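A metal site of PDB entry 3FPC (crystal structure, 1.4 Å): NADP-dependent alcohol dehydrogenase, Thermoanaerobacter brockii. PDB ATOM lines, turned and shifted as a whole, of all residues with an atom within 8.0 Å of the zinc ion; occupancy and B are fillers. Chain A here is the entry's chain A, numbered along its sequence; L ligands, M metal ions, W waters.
Ser 39 touches the zinc ion. Within 4 Å of the zinc ion: Cys 37, Ser 39, His 59 and Asp 150. The nearest printed residue that does not touch the zinc ion is Glu 60 (4.2 Å).
The side-chain sulfur (SG) of Cys 37 lies close to the backbone NH (N) of Ser 39, at 3.4 Å. OG1 of Thr 154 lies within hydrogen-bond range of O of Asp 150 (2.8 Å). ND1 of His 59 sits at hydrogen-bond distance from OG of Ser 113, 2.8 Å away.
The zinc ion is bound by an oxygen (O2) of the ligand (1.9 Å), the side-chain carboxylate of Asp 150 (2.0 Å), a ring nitrogen (NE2) of His 59 (2.0 Å) and the side-chain sulfur of Cys 37 (2.2 Å). The zinc ion has four donor atoms within binding distance.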
ATOM      1  N   ALA A  35      -5.781   8.774  -8.410  1.00  0.00           N
ATOM      2  CA  ALA A  35      -5.437   9.158  -9.764  1.00  0.00           C
ATOM      3  C   ALA A  35      -4.876  10.556  -9.760  1.00  0.00           C
ATOM      4  O   ALA A  35      -5.268  11.358  -8.930  1.00  0.00           O
ATOM      5  CB  ALA A  35      -6.652   9.065 -10.698  1.00  0.00           C
ATOM      6  N   PRO A  36      -3.966  10.858 -10.702  1.00  0.00           N
ATOM      7  CA  PRO A  36      -3.472  12.216 -10.945  1.00  0.00           C
ATOM      8  C   PRO A  36      -4.332  12.959 -11.935  1.00  0.00           C
ATOM      9  O   PRO A  36      -5.047  12.317 -12.694  1.00  0.00           O
ATOM     10  CB  PRO A  36      -2.091  11.975 -11.530  1.00  0.00           C
ATOM     11  CG  PRO A  36      -2.307  10.753 -12.373  1.00  0.00           C
ATOM     12  CD  PRO A  36      -3.277   9.875 -11.564  1.00  0.00           C
ATOM     13  N   CYS A  37      -4.249  14.299 -11.912  1.00  0.00           N
ATOM     14  CA  CYS A  37      -5.105  15.173 -12.679  1.00  0.00           C
ATOM     15  C   CYS A  37      -4.297  16.240 -13.383  1.00  0.00           C
ATOM     16  O   CYS A  37      -3.342  16.776 -12.828  1.00  0.00           O
ATOM     17  CB  CYS A  37      -6.084  15.860 -11.747  1.00  0.00           C
ATOM     18  SG  CYS A  37      -7.373  16.799 -12.596  1.00  0.00           S
ATOM     19  N   THR A  38      -4.734  16.564 -14.585  1.00  0.00           N
ATOM     20  CA  THR A  38      -4.213  17.693 -15.354  1.00  0.00           C
ATOM     21  C   THR A  38      -4.164  18.975 -14.529  1.00  0.00           C
ATOM     22  O   THR A  38      -3.305  19.825 -14.720  1.00  0.00           O
ATOM     23  CB  THR A  38      -5.125  17.943 -16.577  1.00  0.00           C
ATOM     24  OG1 THR A  38      -5.273  16.751 -17.351  1.00  0.00           O
ATOM     25  CG2 THR A  38      -4.575  19.039 -17.458  1.00  0.00           C
ATOM     26  N   SER A  39      -5.150  19.125 -13.631  1.00  0.00           N
ATOM     27  CA  SER A  39      -5.175  20.315 -12.807  1.00  0.00           C
ATOM     28  C   SER A  39      -3.912  20.486 -11.982  1.00  0.00           C
ATOM     29  O   SER A  39      -3.441  21.600 -11.811  1.00  0.00           O
ATOM     30  CB  SER A  39      -6.407  20.318 -11.909  1.00  0.00           C
ATOM     31  OG  SER A  39      -7.552  20.391 -12.690  1.00  0.00           O
ATOM     32  N   ASP A  40      -3.392  19.391 -11.461  1.00  0.00           N
ATOM     33  CA  ASP A  40      -2.142  19.504 -10.698  1.00  0.00           C
ATOM     34  C   ASP A  40      -0.943  19.904 -11.571  1.00  0.00           C
ATOM     35  O   ASP A  40      -0.008  20.565 -11.114  1.00  0.00           O
ATOM     36  CB  ASP A  40      -1.858  18.227  -9.863  1.00  0.00           C
ATOM     37  CG  ASP A  40      -2.698  18.169  -8.585  1.00  0.00           C
ATOM     38  OD1 ASP A  40      -3.430  19.137  -8.235  1.00  0.00           O
ATOM     39  OD2 ASP A  40      -2.619  17.153  -7.897  1.00  0.00           O
ATOM     40  N   GLY A  58      -2.703  15.732  -5.378  1.00  0.00           N
ATOM     41  CA  GLY A  58      -3.746  14.728  -5.607  1.00  0.00           C
ATOM     42  C   GLY A  58      -5.056  15.091  -4.954  1.00  0.00           C
ATOM     43  O   GLY A  58      -5.089  15.590  -3.839  1.00  0.00           O
ATOM     44  N   HIS A  59      -6.156  14.836  -5.657  1.00  0.00           N
ATOM     45  CA  HIS A  59      -7.495  15.094  -5.100  1.00  0.00           C
ATOM     46  C   HIS A  59      -8.536  14.083  -5.593  1.00  0.00           C
ATOM     47  O   HIS A  59      -9.739  14.329  -5.520  1.00  0.00           O
ATOM     48  CB  HIS A  59      -7.931  16.518  -5.393  1.00  0.00           C
ATOM     49  CG  HIS A  59      -7.765  16.914  -6.835  1.00  0.00           C
ATOM     50  ND1 HIS A  59      -6.703  17.690  -7.276  1.00  0.00           N
ATOM     51  CD2 HIS A  59      -8.534  16.667  -7.925  1.00  0.00           C
ATOM     52  CE1 HIS A  59      -6.820  17.858  -8.586  1.00  0.00           C
ATOM     53  NE2 HIS A  59      -7.915  17.244  -9.009  1.00  0.00           N
ATOM     54  N   GLU A  60      -8.071  12.920  -6.070  1.00  0.00           N
ATOM     55  CA  GLU A  60      -8.943  11.827  -6.549  1.00  0.00           C
ATOM     56  C   GLU A  60      -8.547  10.555  -5.847  1.00  0.00           C
ATOM     57  O   GLU A  60      -7.528   9.949  -6.178  1.00  0.00           O
ATOM     58  CB  GLU A  60      -8.804  11.693  -8.077  1.00  0.00           C
ATOM     59  CG  GLU A  60      -9.300  12.906  -8.841  1.00  0.00           C
ATOM     60  CD  GLU A  60      -8.828  12.907 -10.259  1.00  0.00           C
ATOM     61  OE1 GLU A  60      -9.583  12.448 -11.115  1.00  0.00           O
ATOM     62  OE2 GLU A  60      -7.692  13.342 -10.479  1.00  0.00           O
ATOM     63  N   ALA A  85     -13.463  15.329  -4.715  1.00  0.00           N
ATOM     64  CA  ALA A  85     -12.383  16.314  -4.803  1.00  0.00           C
ATOM     65  C   ALA A  85     -12.741  17.614  -4.091  1.00  0.00           C
ATOM     66  O   ALA A  85     -11.847  18.303  -3.606  1.00  0.00           O
ATOM     67  CB  ALA A  85     -12.051  16.597  -6.290  1.00  0.00           C
ATOM     68  N   ILE A  86     -14.032  17.974  -4.115  1.00  0.00           N
ATOM     69  CA  ILE A  86     -14.550  19.168  -3.430  1.00  0.00           C
ATOM     70  C   ILE A  86     -15.190  18.709  -2.119  1.00  0.00           C
ATOM     71  O   ILE A  86     -16.137  17.883  -2.110  1.00  0.00           O
ATOM     72  CB  ILE A  86     -15.514  19.909  -4.382  1.00  0.00           C
ATOM     73  CG1 ILE A  86     -14.751  20.805  -5.386  1.00  0.00           C
ATOM     74  CG2 ILE A  86     -16.533  20.804  -3.616  1.00  0.00           C
ATOM     75  CD1 ILE A  86     -13.578  20.152  -6.196  1.00  0.00           C
ATOM     76  N   TRP A 110     -12.817  23.400  -3.035  1.00  0.00           N
ATOM     77  CA  TRP A 110     -11.770  22.517  -3.540  1.00  0.00           C
ATOM     78  C   TRP A 110     -10.581  22.716  -2.648  1.00  0.00           C
ATOM     79  O   TRP A 110      -9.856  23.686  -2.769  1.00  0.00           O
ATOM     80  CB  TRP A 110     -11.470  22.843  -5.003  1.00  0.00           C
ATOM     81  CG  TRP A 110     -10.261  22.148  -5.558  1.00  0.00           C
ATOM     82  CD1 TRP A 110      -9.774  20.913  -5.220  1.00  0.00           C
ATOM     83  CD2 TRP A 110      -9.384  22.663  -6.560  1.00  0.00           C
ATOM     84  NE1 TRP A 110      -8.641  20.643  -5.952  1.00  0.00           N
ATOM     85  CE2 TRP A 110      -8.366  21.710  -6.763  1.00  0.00           C
ATOM     86  CE3 TRP A 110      -9.354  23.862  -7.300  1.00  0.00           C
ATOM     87  CZ2 TRP A 110      -7.349  21.910  -7.690  1.00  0.00           C
ATOM     88  CZ3 TRP A 110      -8.318  24.062  -8.214  1.00  0.00           C
ATOM     89  CH2 TRP A 110      -7.329  23.100  -8.378  1.00  0.00           C
ATOM     90  N   PHE A 112      -8.261  19.798  -1.315  1.00  0.00           N
ATOM     91  CA  PHE A 112      -7.131  18.941  -1.665  1.00  0.00           C
ATOM     92  C   PHE A 112      -6.359  19.431  -2.899  1.00  0.00           C
ATOM     93  O   PHE A 112      -6.920  19.533  -4.018  1.00  0.00           O
ATOM     94  CB  PHE A 112      -7.644  17.567  -2.043  1.00  0.00           C
ATOM     95  CG  PHE A 112      -8.297  16.773  -0.935  1.00  0.00           C
ATOM     96  CD1 PHE A 112      -7.711  16.597   0.310  1.00  0.00           C
ATOM     97  CD2 PHE A 112      -9.493  16.128  -1.187  1.00  0.00           C
ATOM     98  CE1 PHE A 112      -8.329  15.781   1.274  1.00  0.00           C
ATOM     99  CE2 PHE A 112     -10.089  15.344  -0.237  1.00  0.00           C
ATOM    100  CZ  PHE A 112      -9.519  15.155   0.968  1.00  0.00           C
ATOM    101  N   SER A 113      -5.056  19.696  -2.688  1.00  0.00           N
ATOM    102  CA  SER A 113      -4.133  20.150  -3.734  1.00  0.00           C
ATOM    103  C   SER A 113      -4.408  21.560  -4.254  1.00  0.00           C
ATOM    104  O   SER A 113      -3.871  21.971  -5.261  1.00  0.00           O
ATOM    105  CB  SER A 113      -3.863  19.095  -4.852  1.00  0.00           C
ATOM    106  OG  SER A 113      -4.784  19.159  -5.901  1.00  0.00           O
ATOM    107  N   PRO A 149     -14.846  11.066  -7.993  1.00  0.00           N
ATOM    108  CA  PRO A 149     -14.527  12.315  -7.270  1.00  0.00           C
ATOM    109  C   PRO A 149     -14.335  13.592  -8.051  1.00  0.00           C
ATOM    110  O   PRO A 149     -14.584  14.656  -7.519  1.00  0.00           O
ATOM    111  CB  PRO A 149     -13.198  11.972  -6.599  1.00  0.00           C
ATOM    112  CG  PRO A 149     -13.339  10.521  -6.276  1.00  0.00           C
ATOM    113  CD  PRO A 149     -13.972   9.973  -7.530  1.00  0.00           C
ATOM    114  N   ASP A 150     -13.909  13.467  -9.294  1.00  0.00           N
ATOM    115  CA  ASP A 150     -13.528  14.620 -10.121  1.00  0.00           C
ATOM    116  C   ASP A 150     -13.960  14.434 -11.557  1.00  0.00           C
ATOM    117  O   ASP A 150     -14.650  15.281 -12.111  1.00  0.00           O
ATOM    118  CB  ASP A 150     -12.027  14.771 -10.009  1.00  0.00           C
ATOM    119  CG  ASP A 150     -11.493  16.055 -10.567  1.00  0.00           C
ATOM    120  OD1 ASP A 150     -12.250  16.854 -11.143  1.00  0.00           O
ATOM    121  OD2 ASP A 150     -10.268  16.252 -10.404  1.00  0.00           O
ATOM    122  N   MET A 151     -13.546  13.348 -12.215  1.00  0.00           N
ATOM    123  CA  MET A 151     -13.823  13.261 -13.665  1.00  0.00           C
ATOM    124  C   MET A 151     -15.303  13.275 -13.999  1.00  0.00           C
ATOM    125  O   MET A 151     -15.790  14.033 -14.842  1.00  0.00           O
ATOM    126  CB  MET A 151     -13.148  12.040 -14.294  1.00  0.00           C
ATOM    127  CG  MET A 151     -11.642  12.036 -14.179  1.00  0.00           C
ATOM    128  SD  MET A 151     -10.782  13.415 -14.944  1.00  0.00           S
ATOM    129  CE  MET A 151     -10.711  14.656 -13.611  1.00  0.00           C
ATOM    130  N   THR A 154     -17.047  16.663 -12.682  1.00  0.00           N
ATOM    131  CA  THR A 154     -16.659  17.813 -13.465  1.00  0.00           C
ATOM    132  C   THR A 154     -17.242  17.708 -14.902  1.00  0.00           C
ATOM    133  O   THR A 154     -17.833  18.644 -15.414  1.00  0.00           O
ATOM    134  CB  THR A 154     -15.151  17.958 -13.526  1.00  0.00           C
ATOM    135  OG1 THR A 154     -14.614  18.070 -12.208  1.00  0.00           O
ATOM    136  CG2 THR A 154     -14.751  19.223 -14.336  1.00  0.00           C
ATOM    137  N   VAL A 178     -12.268  14.539 -18.703  1.00  0.00           N
ATOM    138  CA  VAL A 178     -13.406  15.416 -18.341  1.00  0.00           C
ATOM    139  C   VAL A 178     -14.358  15.550 -19.520  1.00  0.00           C
ATOM    140  O   VAL A 178     -15.576  15.394 -19.367  1.00  0.00           O
ATOM    141  CB  VAL A 178     -12.939  16.783 -17.822  1.00  0.00           C
ATOM    142  CG1 VAL A 178     -14.074  17.792 -17.689  1.00  0.00           C
ATOM    143  CG2 VAL A 178     -12.205  16.616 -16.468  1.00  0.00           C
ATOM    144  N   TYR A 267     -10.002  24.136 -16.365  1.00  0.00           N
ATOM    145  CA  TYR A 267      -9.110  24.953 -15.548  1.00  0.00           C
ATOM    146  C   TYR A 267      -8.107  25.606 -16.489  1.00  0.00           C
ATOM    147  O   TYR A 267      -7.297  24.961 -17.106  1.00  0.00           O
ATOM    148  CB  TYR A 267      -8.495  24.048 -14.498  1.00  0.00           C
ATOM    149  CG  TYR A 267      -7.384  24.557 -13.600  1.00  0.00           C
ATOM    150  CD1 TYR A 267      -6.906  25.845 -13.608  1.00  0.00           C
ATOM    151  CD2 TYR A 267      -6.797  23.685 -12.725  1.00  0.00           C
ATOM    152  CE1 TYR A 267      -5.858  26.203 -12.767  1.00  0.00           C
ATOM    153  CE2 TYR A 267      -5.762  24.037 -11.882  1.00  0.00           C
ATOM    154  CZ  TYR A 267      -5.274  25.291 -11.928  1.00  0.00           C
ATOM    155  OH  TYR A 267      -4.212  25.666 -11.098  1.00  0.00           O
ATOM    156  N   LEU A 294     -16.466  25.395 -11.139  1.00  0.00           N
ATOM    157  CA  LEU A 294     -15.877  24.292 -10.407  1.00  0.00           C
ATOM    158  C   LEU A 294     -16.883  23.199 -10.128  1.00  0.00           C
ATOM    159  O   LEU A 294     -18.027  23.471  -9.805  1.00  0.00           O
ATOM    160  CB  LEU A 294     -15.310  24.846  -9.098  1.00  0.00           C
ATOM    161  CG  LEU A 294     -14.618  23.894  -8.104  1.00  0.00           C
ATOM    162  CD1 LEU A 294     -13.361  23.339  -8.728  1.00  0.00           C
ATOM    163  CD2 LEU A 294     -14.247  24.662  -6.820  1.00  0.00           C
ATOM    164  N   CYS A 295     -16.457  21.941 -10.191  1.00  0.00           N
ATOM    165  CA  CYS A 295     -17.383  20.832 -10.010  1.00  0.00           C
ATOM    166  C   CYS A 295     -18.027  20.786  -8.614  1.00  0.00           C
ATOM    167  O   CYS A 295     -17.395  21.122  -7.613  1.00  0.00           O
ATOM    168  CB  CYS A 295     -16.706  19.489 -10.253  1.00  0.00           C
ATOM    169  SG  CYS A 295     -15.341  19.113  -9.162  1.00  0.00           S
ATOM    170  N   LYS A 346      -6.770   8.450 -18.493  1.00  0.00           N
ATOM    171  CA  LYS A 346      -6.503   8.639 -17.087  1.00  0.00           C
ATOM    172  C   LYS A 346      -5.716   7.431 -16.476  1.00  0.00           C
ATOM    173  O   LYS A 346      -6.096   6.287 -16.715  1.00  0.00           O
ATOM    174  CB  LYS A 346      -7.852   8.726 -16.416  1.00  0.00           C
ATOM    175  CG  LYS A 346      -7.830   9.242 -15.106  1.00  0.00           C
ATOM    176  CD  LYS A 346      -7.633  10.766 -15.058  1.00  0.00           C
ATOM    177  CE  LYS A 346      -8.102  11.199 -13.695  1.00  0.00           C
ATOM    178  NZ  LYS A 346      -7.696  12.571 -13.344  1.00  0.00           N
HETATM  179 AS1  LIG L   1     -10.656  19.981 -10.553  1.00  0.00          AS
HETATM  180  O1  LIG L   1     -11.938  19.411 -11.614  1.00  0.00           O
HETATM  181  O2  LIG L   1      -9.253  19.208 -11.075  1.00  0.00           O
HETATM  182  C1  LIG L   1     -10.441  21.872 -10.715  1.00  0.00           C
HETATM  183  C2  LIG L   1     -11.085  19.522  -8.713  1.00  0.00           C
HETATM  184 ZN    ZN M   1      -8.717  17.350 -10.879  1.00  0.00          ZN
HETATM  185  O   HOH W   1     -10.643  17.916 -13.672  1.00  0.00           O
